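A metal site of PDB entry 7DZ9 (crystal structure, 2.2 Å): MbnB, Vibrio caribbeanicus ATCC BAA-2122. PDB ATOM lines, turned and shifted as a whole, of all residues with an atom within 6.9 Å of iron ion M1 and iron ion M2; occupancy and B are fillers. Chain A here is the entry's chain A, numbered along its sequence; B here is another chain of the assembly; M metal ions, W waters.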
ATOM      1  N   GLU A  29      28.034  18.948  -8.263  1.00  0.00           N
ATOM      2  CA  GLU A  29      27.044  19.583  -7.397  1.00  0.00           C
ATOM      3  C   GLU A  29      27.736  20.648  -6.567  1.00  0.00           C
ATOM      4  O   GLU A  29      28.486  20.331  -5.645  1.00  0.00           O
ATOM      5  CB  GLU A  29      26.367  18.553  -6.499  1.00  0.00           C
ATOM      6  CG  GLU A  29      25.117  19.119  -5.821  1.00  0.00           C
ATOM      7  CD  GLU A  29      24.608  18.226  -4.705  1.00  0.00           C
ATOM      8  OE1 GLU A  29      23.634  17.475  -4.935  1.00  0.00           O
ATOM      9  OE2 GLU A  29      25.193  18.281  -3.592  1.00  0.00           O
ATOM     10  N   LEU A  31      27.890  23.334  -3.686  1.00  0.00           N
ATOM     11  CA  LEU A  31      27.228  23.876  -2.495  1.00  0.00           C
ATOM     12  C   LEU A  31      27.100  25.379  -2.731  1.00  0.00           C
ATOM     13  O   LEU A  31      27.939  26.191  -2.338  1.00  0.00           O
ATOM     14  CB  LEU A  31      28.015  23.531  -1.235  1.00  0.00           C
ATOM     15  CG  LEU A  31      27.222  23.541   0.076  1.00  0.00           C
ATOM     16  CD1 LEU A  31      26.121  22.463   0.066  1.00  0.00           C
ATOM     17  CD2 LEU A  31      28.147  23.353   1.290  1.00  0.00           C
ATOM     18  N   HIS A  55      23.209  22.684  -4.480  1.00  0.00           N
ATOM     19  CA  HIS A  55      22.895  22.188  -3.150  1.00  0.00           C
ATOM     20  C   HIS A  55      23.103  23.347  -2.179  1.00  0.00           C
ATOM     21  O   HIS A  55      24.191  23.900  -2.119  1.00  0.00           O
ATOM     22  CB  HIS A  55      23.815  21.020  -2.809  1.00  0.00           C
ATOM     23  CG  HIS A  55      23.367  20.189  -1.649  1.00  0.00           C
ATOM     24  ND1 HIS A  55      22.060  19.785  -1.472  1.00  0.00           N
ATOM     25  CD2 HIS A  55      24.079  19.627  -0.645  1.00  0.00           C
ATOM     26  CE1 HIS A  55      21.979  19.047  -0.378  1.00  0.00           C
ATOM     27  NE2 HIS A  55      23.188  18.929   0.141  1.00  0.00           N
ATOM     28  N   ILE A  56      22.072  23.682  -1.385  1.00  0.00           N
ATOM     29  CA  ILE A  56      22.104  24.840  -0.498  1.00  0.00           C
ATOM     30  C   ILE A  56      22.246  24.345   0.937  1.00  0.00           C
ATOM     31  O   ILE A  56      21.397  23.579   1.417  1.00  0.00           O
ATOM     32  CB  ILE A  56      20.861  25.717  -0.650  1.00  0.00           C
ATOM     33  CG1 ILE A  56      20.669  26.150  -2.094  1.00  0.00           C
ATOM     34  CG2 ILE A  56      20.901  26.927   0.309  1.00  0.00           C
ATOM     35  CD1 ILE A  56      19.221  26.512  -2.391  1.00  0.00           C
ATOM     36  N   MET A  57      23.309  24.757   1.609  1.00  0.00           N
ATOM     37  CA  MET A  57      23.603  24.343   2.978  1.00  0.00           C
ATOM     38  C   MET A  57      22.990  25.269   4.026  1.00  0.00           C
ATOM     39  O   MET A  57      22.359  24.792   4.987  1.00  0.00           O
ATOM     40  CB  MET A  57      25.126  24.280   3.167  1.00  0.00           C
ATOM     41  CG  MET A  57      25.563  24.280   4.618  1.00  0.00           C
ATOM     42  SD  MET A  57      24.915  22.836   5.465  1.00  0.00           S
ATOM     43  CE  MET A  57      25.539  21.633   4.391  1.00  0.00           C
ATOM     44  N   ASP A  90      17.941  21.862  -1.068  1.00  0.00           N
ATOM     45  CA  ASP A  90      18.254  22.420   0.247  1.00  0.00           C
ATOM     46  C   ASP A  90      18.030  21.320   1.287  1.00  0.00           C
ATOM     47  O   ASP A  90      17.728  20.166   0.957  1.00  0.00           O
ATOM     48  CB  ASP A  90      17.397  23.665   0.525  1.00  0.00           C
ATOM     49  CG  ASP A  90      18.017  24.627   1.563  1.00  0.00           C
ATOM     50  OD1 ASP A  90      18.704  24.180   2.508  1.00  0.00           O
ATOM     51  OD2 ASP A  90      17.778  25.848   1.453  1.00  0.00           O
ATOM     52  N   HIS A  91      18.183  21.683   2.559  1.00  0.00           N
ATOM     53  CA  HIS A  91      18.115  20.750   3.674  1.00  0.00           C
ATOM     54  C   HIS A  91      16.930  21.055   4.571  1.00  0.00           C
ATOM     55  O   HIS A  91      16.407  22.170   4.594  1.00  0.00           O
ATOM     56  CB  HIS A  91      19.378  20.835   4.538  1.00  0.00           C
ATOM     57  CG  HIS A  91      20.621  20.442   3.812  1.00  0.00           C
ATOM     58  ND1 HIS A  91      21.252  21.277   2.916  1.00  0.00           N
ATOM     59  CD2 HIS A  91      21.338  19.292   3.829  1.00  0.00           C
ATOM     60  CE1 HIS A  91      22.317  20.659   2.428  1.00  0.00           C
ATOM     61  NE2 HIS A  91      22.392  19.460   2.969  1.00  0.00           N
ATOM     62  N   MET A 105      24.440  21.397  12.051  1.00  0.00           N
ATOM     63  CA  MET A 105      23.038  21.310  11.659  1.00  0.00           C
ATOM     64  C   MET A 105      22.422  20.079  12.320  1.00  0.00           C
ATOM     65  O   MET A 105      22.860  18.953  12.053  1.00  0.00           O
ATOM     66  CB  MET A 105      22.899  21.243  10.136  1.00  0.00           C
ATOM     67  CG  MET A 105      21.453  21.404   9.584  1.00  0.00           C
ATOM     68  SD  MET A 105      21.305  21.218   7.754  1.00  0.00           S
ATOM     69  CE  MET A 105      21.361  19.443   7.594  1.00  0.00           C
ATOM     70  N   GLU A 135      16.635  17.308   1.004  1.00  0.00           N
ATOM     71  CA  GLU A 135      17.414  16.114   1.305  1.00  0.00           C
ATOM     72  C   GLU A 135      17.022  15.512   2.651  1.00  0.00           C
ATOM     73  O   GLU A 135      16.807  16.230   3.637  1.00  0.00           O
ATOM     74  CB  GLU A 135      18.915  16.436   1.309  1.00  0.00           C
ATOM     75  CG  GLU A 135      19.785  15.235   1.586  1.00  0.00           C
ATOM     76  CD  GLU A 135      21.286  15.557   1.590  1.00  0.00           C
ATOM     77  OE1 GLU A 135      21.636  16.744   1.586  1.00  0.00           O
ATOM     78  OE2 GLU A 135      22.095  14.605   1.629  1.00  0.00           O
ATOM     79  N   ASN A 136      16.930  14.177   2.703  1.00  0.00           N
ATOM     80  CA  ASN A 136      16.694  13.472   3.969  1.00  0.00           C
ATOM     81  C   ASN A 136      17.900  13.569   4.888  1.00  0.00           C
ATOM     82  O   ASN A 136      19.053  13.486   4.455  1.00  0.00           O
ATOM     83  CB  ASN A 136      16.336  12.005   3.711  1.00  0.00           C
ATOM     84  CG  ASN A 136      17.357  11.283   2.831  1.00  0.00           C
ATOM     85  OD1 ASN A 136      17.625  11.701   1.704  1.00  0.00           O
ATOM     86  ND2 ASN A 136      17.915  10.177   3.342  1.00  0.00           N
ATOM     87  N   LEU A 163      15.424  14.896  -2.719  1.00  0.00           N
ATOM     88  CA  LEU A 163      16.793  14.512  -3.031  1.00  0.00           C
ATOM     89  C   LEU A 163      17.173  13.410  -2.051  1.00  0.00           C
ATOM     90  O   LEU A 163      17.342  13.677  -0.849  1.00  0.00           O
ATOM     91  CB  LEU A 163      17.739  15.713  -2.931  1.00  0.00           C
ATOM     92  CG  LEU A 163      19.255  15.458  -3.095  1.00  0.00           C
ATOM     93  CD1 LEU A 163      19.589  14.981  -4.494  1.00  0.00           C
ATOM     94  CD2 LEU A 163      20.054  16.723  -2.762  1.00  0.00           C
ATOM     95  N   PHE A 164      17.275  12.167  -2.534  1.00  0.00           N
ATOM     96  CA  PHE A 164      17.385  11.043  -1.622  1.00  0.00           C
ATOM     97  C   PHE A 164      18.849  10.686  -1.406  1.00  0.00           C
ATOM     98  O   PHE A 164      19.542  10.287  -2.348  1.00  0.00           O
ATOM     99  CB  PHE A 164      16.635   9.815  -2.122  1.00  0.00           C
ATOM    100  CG  PHE A 164      16.649   8.669  -1.154  1.00  0.00           C
ATOM    101  CD1 PHE A 164      15.998   8.763   0.089  1.00  0.00           C
ATOM    102  CD2 PHE A 164      17.307   7.490  -1.476  1.00  0.00           C
ATOM    103  CE1 PHE A 164      16.000   7.698   0.974  1.00  0.00           C
ATOM    104  CE2 PHE A 164      17.317   6.414  -0.588  1.00  0.00           C
ATOM    105  CZ  PHE A 164      16.652   6.520   0.639  1.00  0.00           C
ATOM    106  N   ASP A 165      19.315  10.817  -0.177  1.00  0.00           N
ATOM    107  CA  ASP A 165      20.670  10.484   0.194  1.00  0.00           C
ATOM    108  C   ASP A 165      20.667   9.055   0.720  1.00  0.00           C
ATOM    109  O   ASP A 165      20.103   8.772   1.779  1.00  0.00           O
ATOM    110  CB  ASP A 165      21.220  11.469   1.230  1.00  0.00           C
ATOM    111  CG  ASP A 165      22.730  11.328   1.453  1.00  0.00           C
ATOM    112  OD1 ASP A 165      23.192  10.213   1.758  1.00  0.00           O
ATOM    113  OD2 ASP A 165      23.460  12.340   1.357  1.00  0.00           O
ATOM    114  N   ILE A 166      21.302   8.163  -0.042  1.00  0.00           N
ATOM    115  CA  ILE A 166      21.258   6.735   0.242  1.00  0.00           C
ATOM    116  C   ILE A 166      21.984   6.402   1.534  1.00  0.00           C
ATOM    117  O   ILE A 166      21.522   5.574   2.334  1.00  0.00           O
ATOM    118  CB  ILE A 166      21.838   5.963  -0.955  1.00  0.00           C
ATOM    119  CG1 ILE A 166      20.951   6.185  -2.202  1.00  0.00           C
ATOM    120  CG2 ILE A 166      22.002   4.487  -0.615  1.00  0.00           C
ATOM    121  CD1 ILE A 166      21.464   5.486  -3.446  1.00  0.00           C
ATOM    122  N   SER A 167      23.143   7.018   1.778  1.00  0.00           N
ATOM    123  CA  SER A 167      23.860   6.685   2.995  1.00  0.00           C
ATOM    124  C   SER A 167      23.261   7.389   4.212  1.00  0.00           C
ATOM    125  O   SER A 167      23.328   6.838   5.315  1.00  0.00           O
ATOM    126  CB  SER A 167      25.362   6.993   2.854  1.00  0.00           C
ATOM    127  OG  SER A 167      25.623   8.315   2.393  1.00  0.00           O
ATOM    128  N   ASN A 168      22.663   8.584   4.049  1.00  0.00           N
ATOM    129  CA  ASN A 168      21.903   9.182   5.143  1.00  0.00           C
ATOM    130  C   ASN A 168      20.794   8.262   5.620  1.00  0.00           C
ATOM    131  O   ASN A 168      20.570   8.112   6.823  1.00  0.00           O
ATOM    132  CB  ASN A 168      21.286  10.516   4.711  1.00  0.00           C
ATOM    133  CG  ASN A 168      22.314  11.602   4.521  1.00  0.00           C
ATOM    134  OD1 ASN A 168      23.519  11.349   4.536  1.00  0.00           O
ATOM    135  ND2 ASN A 168      21.829  12.814   4.274  1.00  0.00           N
ATOM    136  N   HIS A 194      22.227  11.098  -3.601  1.00  0.00           N
ATOM    137  CA  HIS A 194      23.525  11.242  -2.951  1.00  0.00           C
ATOM    138  C   HIS A 194      23.975   9.892  -2.400  1.00  0.00           C
ATOM    139  O   HIS A 194      23.166   9.056  -1.987  1.00  0.00           O
ATOM    140  CB  HIS A 194      23.463  12.222  -1.763  1.00  0.00           C
ATOM    141  CG  HIS A 194      23.469  13.677  -2.113  1.00  0.00           C
ATOM    142  ND1 HIS A 194      23.549  14.655  -1.144  1.00  0.00           N
ATOM    143  CD2 HIS A 194      23.381  14.332  -3.293  1.00  0.00           C
ATOM    144  CE1 HIS A 194      23.526  15.844  -1.721  1.00  0.00           C
ATOM    145  NE2 HIS A 194      23.427  15.674  -3.025  1.00  0.00           N
ATOM    146  N   ILE A 195      25.287   9.703  -2.285  1.00  0.00           N
ATOM    147  CA  ILE A 195      25.830   8.543  -1.586  1.00  0.00           C
ATOM    148  C   ILE A 195      27.217   8.900  -1.095  1.00  0.00           C
ATOM    149  O   ILE A 195      27.962   9.618  -1.780  1.00  0.00           O
ATOM    150  CB  ILE A 195      25.819   7.289  -2.490  1.00  0.00           C
ATOM    151  CG1 ILE A 195      25.947   5.996  -1.663  1.00  0.00           C
ATOM    152  CG2 ILE A 195      26.906   7.363  -3.574  1.00  0.00           C
ATOM    153  CD1 ILE A 195      25.909   4.718  -2.532  1.00  0.00           C
ATOM    154  N   ALA A 196      27.568   8.420   0.087  1.00  0.00           N
ATOM    155  CA  ALA A 196      28.822   8.826   0.722  1.00  0.00           C
ATOM    156  C   ALA A 196      29.233   7.813   1.788  1.00  0.00           C
ATOM    157  O   ALA A 196      28.545   6.818   2.031  1.00  0.00           O
ATOM    158  CB  ALA A 196      28.702  10.219   1.345  1.00  0.00           C
ATOM    159  N   ASP A 209      27.629  11.305   9.898  1.00  0.00           N
ATOM    160  CA  ASP A 209      27.526  11.508   8.447  1.00  0.00           C
ATOM    161  C   ASP A 209      28.653  12.435   7.953  1.00  0.00           C
ATOM    162  O   ASP A 209      28.414  13.556   7.516  1.00  0.00           O
ATOM    163  CB  ASP A 209      26.166  12.076   8.086  1.00  0.00           C
ATOM    164  CG  ASP A 209      25.970  12.213   6.592  1.00  0.00           C
ATOM    165  OD1 ASP A 209      26.514  11.369   5.840  1.00  0.00           O
ATOM    166  OD2 ASP A 209      25.308  13.168   6.157  1.00  0.00           O
ATOM    167  N   HIS A 211      31.031  12.128   5.424  1.00  0.00           N
ATOM    168  CA  HIS A 211      31.499  12.197   4.040  1.00  0.00           C
ATOM    169  C   HIS A 211      33.036  12.164   3.969  1.00  0.00           C
ATOM    170  O   HIS A 211      33.667  12.912   3.227  1.00  0.00           O
ATOM    171  CB  HIS A 211      30.952  13.438   3.333  1.00  0.00           C
ATOM    172  CG  HIS A 211      29.461  13.563   3.378  1.00  0.00           C
ATOM    173  ND1 HIS A 211      28.786  14.727   3.069  1.00  0.00           N
ATOM    174  CD2 HIS A 211      28.494  12.663   3.718  1.00  0.00           C
ATOM    175  CE1 HIS A 211      27.490  14.544   3.198  1.00  0.00           C
ATOM    176  NE2 HIS A 211      27.284  13.301   3.596  1.00  0.00           N
ATOM    177  N   SER A 236      25.372  11.922  -6.821  1.00  0.00           N
ATOM    178  CA  SER A 236      26.578  12.635  -6.436  1.00  0.00           C
ATOM    179  C   SER A 236      27.262  11.806  -5.355  1.00  0.00           C
ATOM    180  O   SER A 236      26.639  11.440  -4.359  1.00  0.00           O
ATOM    181  CB  SER A 236      26.236  14.036  -5.911  1.00  0.00           C
ATOM    182  OG  SER A 236      27.319  14.607  -5.215  1.00  0.00           O
ATOM    183  N   GLU A 238      29.622  11.905  -2.530  1.00  0.00           N
ATOM    184  CA  GLU A 238      30.039  13.050  -1.726  1.00  0.00           C
ATOM    185  C   GLU A 238      31.361  12.825  -1.018  1.00  0.00           C
ATOM    186  O   GLU A 238      31.656  11.714  -0.585  1.00  0.00           O
ATOM    187  CB  GLU A 238      28.973  13.388  -0.680  1.00  0.00           C
ATOM    188  CG  GLU A 238      27.562  13.472  -1.215  1.00  0.00           C
ATOM    189  CD  GLU A 238      26.643  14.198  -0.252  1.00  0.00           C
ATOM    190  OE1 GLU A 238      25.923  13.508   0.501  1.00  0.00           O
ATOM    191  OE2 GLU A 238      26.620  15.444  -0.258  1.00  0.00           O
ATOM    192  N   THR B  17      30.364  22.682   5.121  1.00  0.00           N
ATOM    193  CA  THR B  17      30.226  21.445   4.355  1.00  0.00           C
ATOM    194  C   THR B  17      29.047  20.661   4.895  1.00  0.00           C
ATOM    195  O   THR B  17      28.611  20.865   6.024  1.00  0.00           O
ATOM    196  CB  THR B  17      31.491  20.572   4.441  1.00  0.00           C
ATOM    197  OG1 THR B  17      31.723  20.221   5.806  1.00  0.00           O
ATOM    198  CG2 THR B  17      32.716  21.306   3.867  1.00  0.00           C
ATOM    199  N   CYS B  18      28.565  19.720   4.074  1.00  0.00           N
ATOM    200  CA  CYS B  18      27.490  18.854   4.536  1.00  0.00           C
ATOM    201  C   CYS B  18      27.989  17.791   5.497  1.00  0.00           C
ATOM    202  O   CYS B  18      27.243  17.374   6.387  1.00  0.00           O
ATOM    203  CB  CYS B  18      26.838  18.148   3.342  1.00  0.00           C
ATOM    204  SG  CYS B  18      25.637  19.099   2.453  1.00  0.00           S
ATOM    205  N   GLY B  19      29.258  17.410   5.375  1.00  0.00           N
ATOM    206  CA  GLY B  19      29.882  16.475   6.278  1.00  0.00           C
ATOM    207  C   GLY B  19      29.864  16.935   7.711  1.00  0.00           C
ATOM    208  O   GLY B  19      30.356  18.023   8.041  1.00  0.00           O
HETATM  209 FE    FE M   1      23.512  17.732   2.055  1.00  0.00          FE
HETATM  210 FE    FE M   2      23.948  14.268   1.123  1.00  0.00          FE
HETATM  211 FE    FE M   3      25.335  12.556   4.069  1.00  0.00          FE
HETATM  212  O   HOH W   1      23.556  16.655   4.252  1.00  0.00           O
HETATM  213  O   HOH W   2      24.616  16.320   1.100  1.00  0.00           O
HETATM  214  O   HOH W   3      24.188  14.217   3.105  1.00  0.00           O
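The side-chain carboxylate (OE2) of Glu 135 binds iron ion M2. Water W3 binds iron ion M2 (2.0 Å). OD2 of Asp 165 binds iron ion M2 (2.0 Å). Iron ion M2 is bound by water W2 (2.2 Å). OE1 of Glu 238 is bound to iron ion M2 (2.2 Å). ND1 of His 194 binds iron ion M2 (2.3 Å).
The nearest printed residue that does not touch iron ion M1 is His 194 (4.2 Å).
Iron ion M1 is bound by water W2, OE1 of Glu 135, NE2 of His 91, NE2 of His 55, water W1 and SG of Cys 18 of chain B.
N of Glu 135 is in hydrogen-bond range of O of Asp 90. A ring nitrogen (ND1) of His 91 is in hydrogen-bond range of the backbone carbonyl oxygen (O) of Ile 56 (2.8 Å). The backbone NH (N) of Asn 168 sits at hydrogen-bond distance from the side-chain carboxylate (OD1) of Asp 165 (2.9 Å). The backbone NH (N) of Ile 166 sits at hydrogen-bond distance from the backbone carbonyl oxygen (O) of His 194 (2.8 Å). The backbone NH of Asp 165 sits at hydrogen-bond distance from the side-chain amide oxygen of Asn 136, at 2.7 Å. NE2 of His 194 is in hydrogen-bond range of OE1 of Glu 29. O of Ile 195 sits at hydrogen-bond distance from N of Glu 238 (2.9 Å). OE2 of Glu 135 sits close to ND2 of Asn 168 (3.2 Å).
Four residues have an atom within 4 Å of iron ion M2: Glu 135, Asp 165, His 194 and Glu 238. The nearest printed residue that does not touch iron ion M2 is Asn 168 (4.1 Å).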
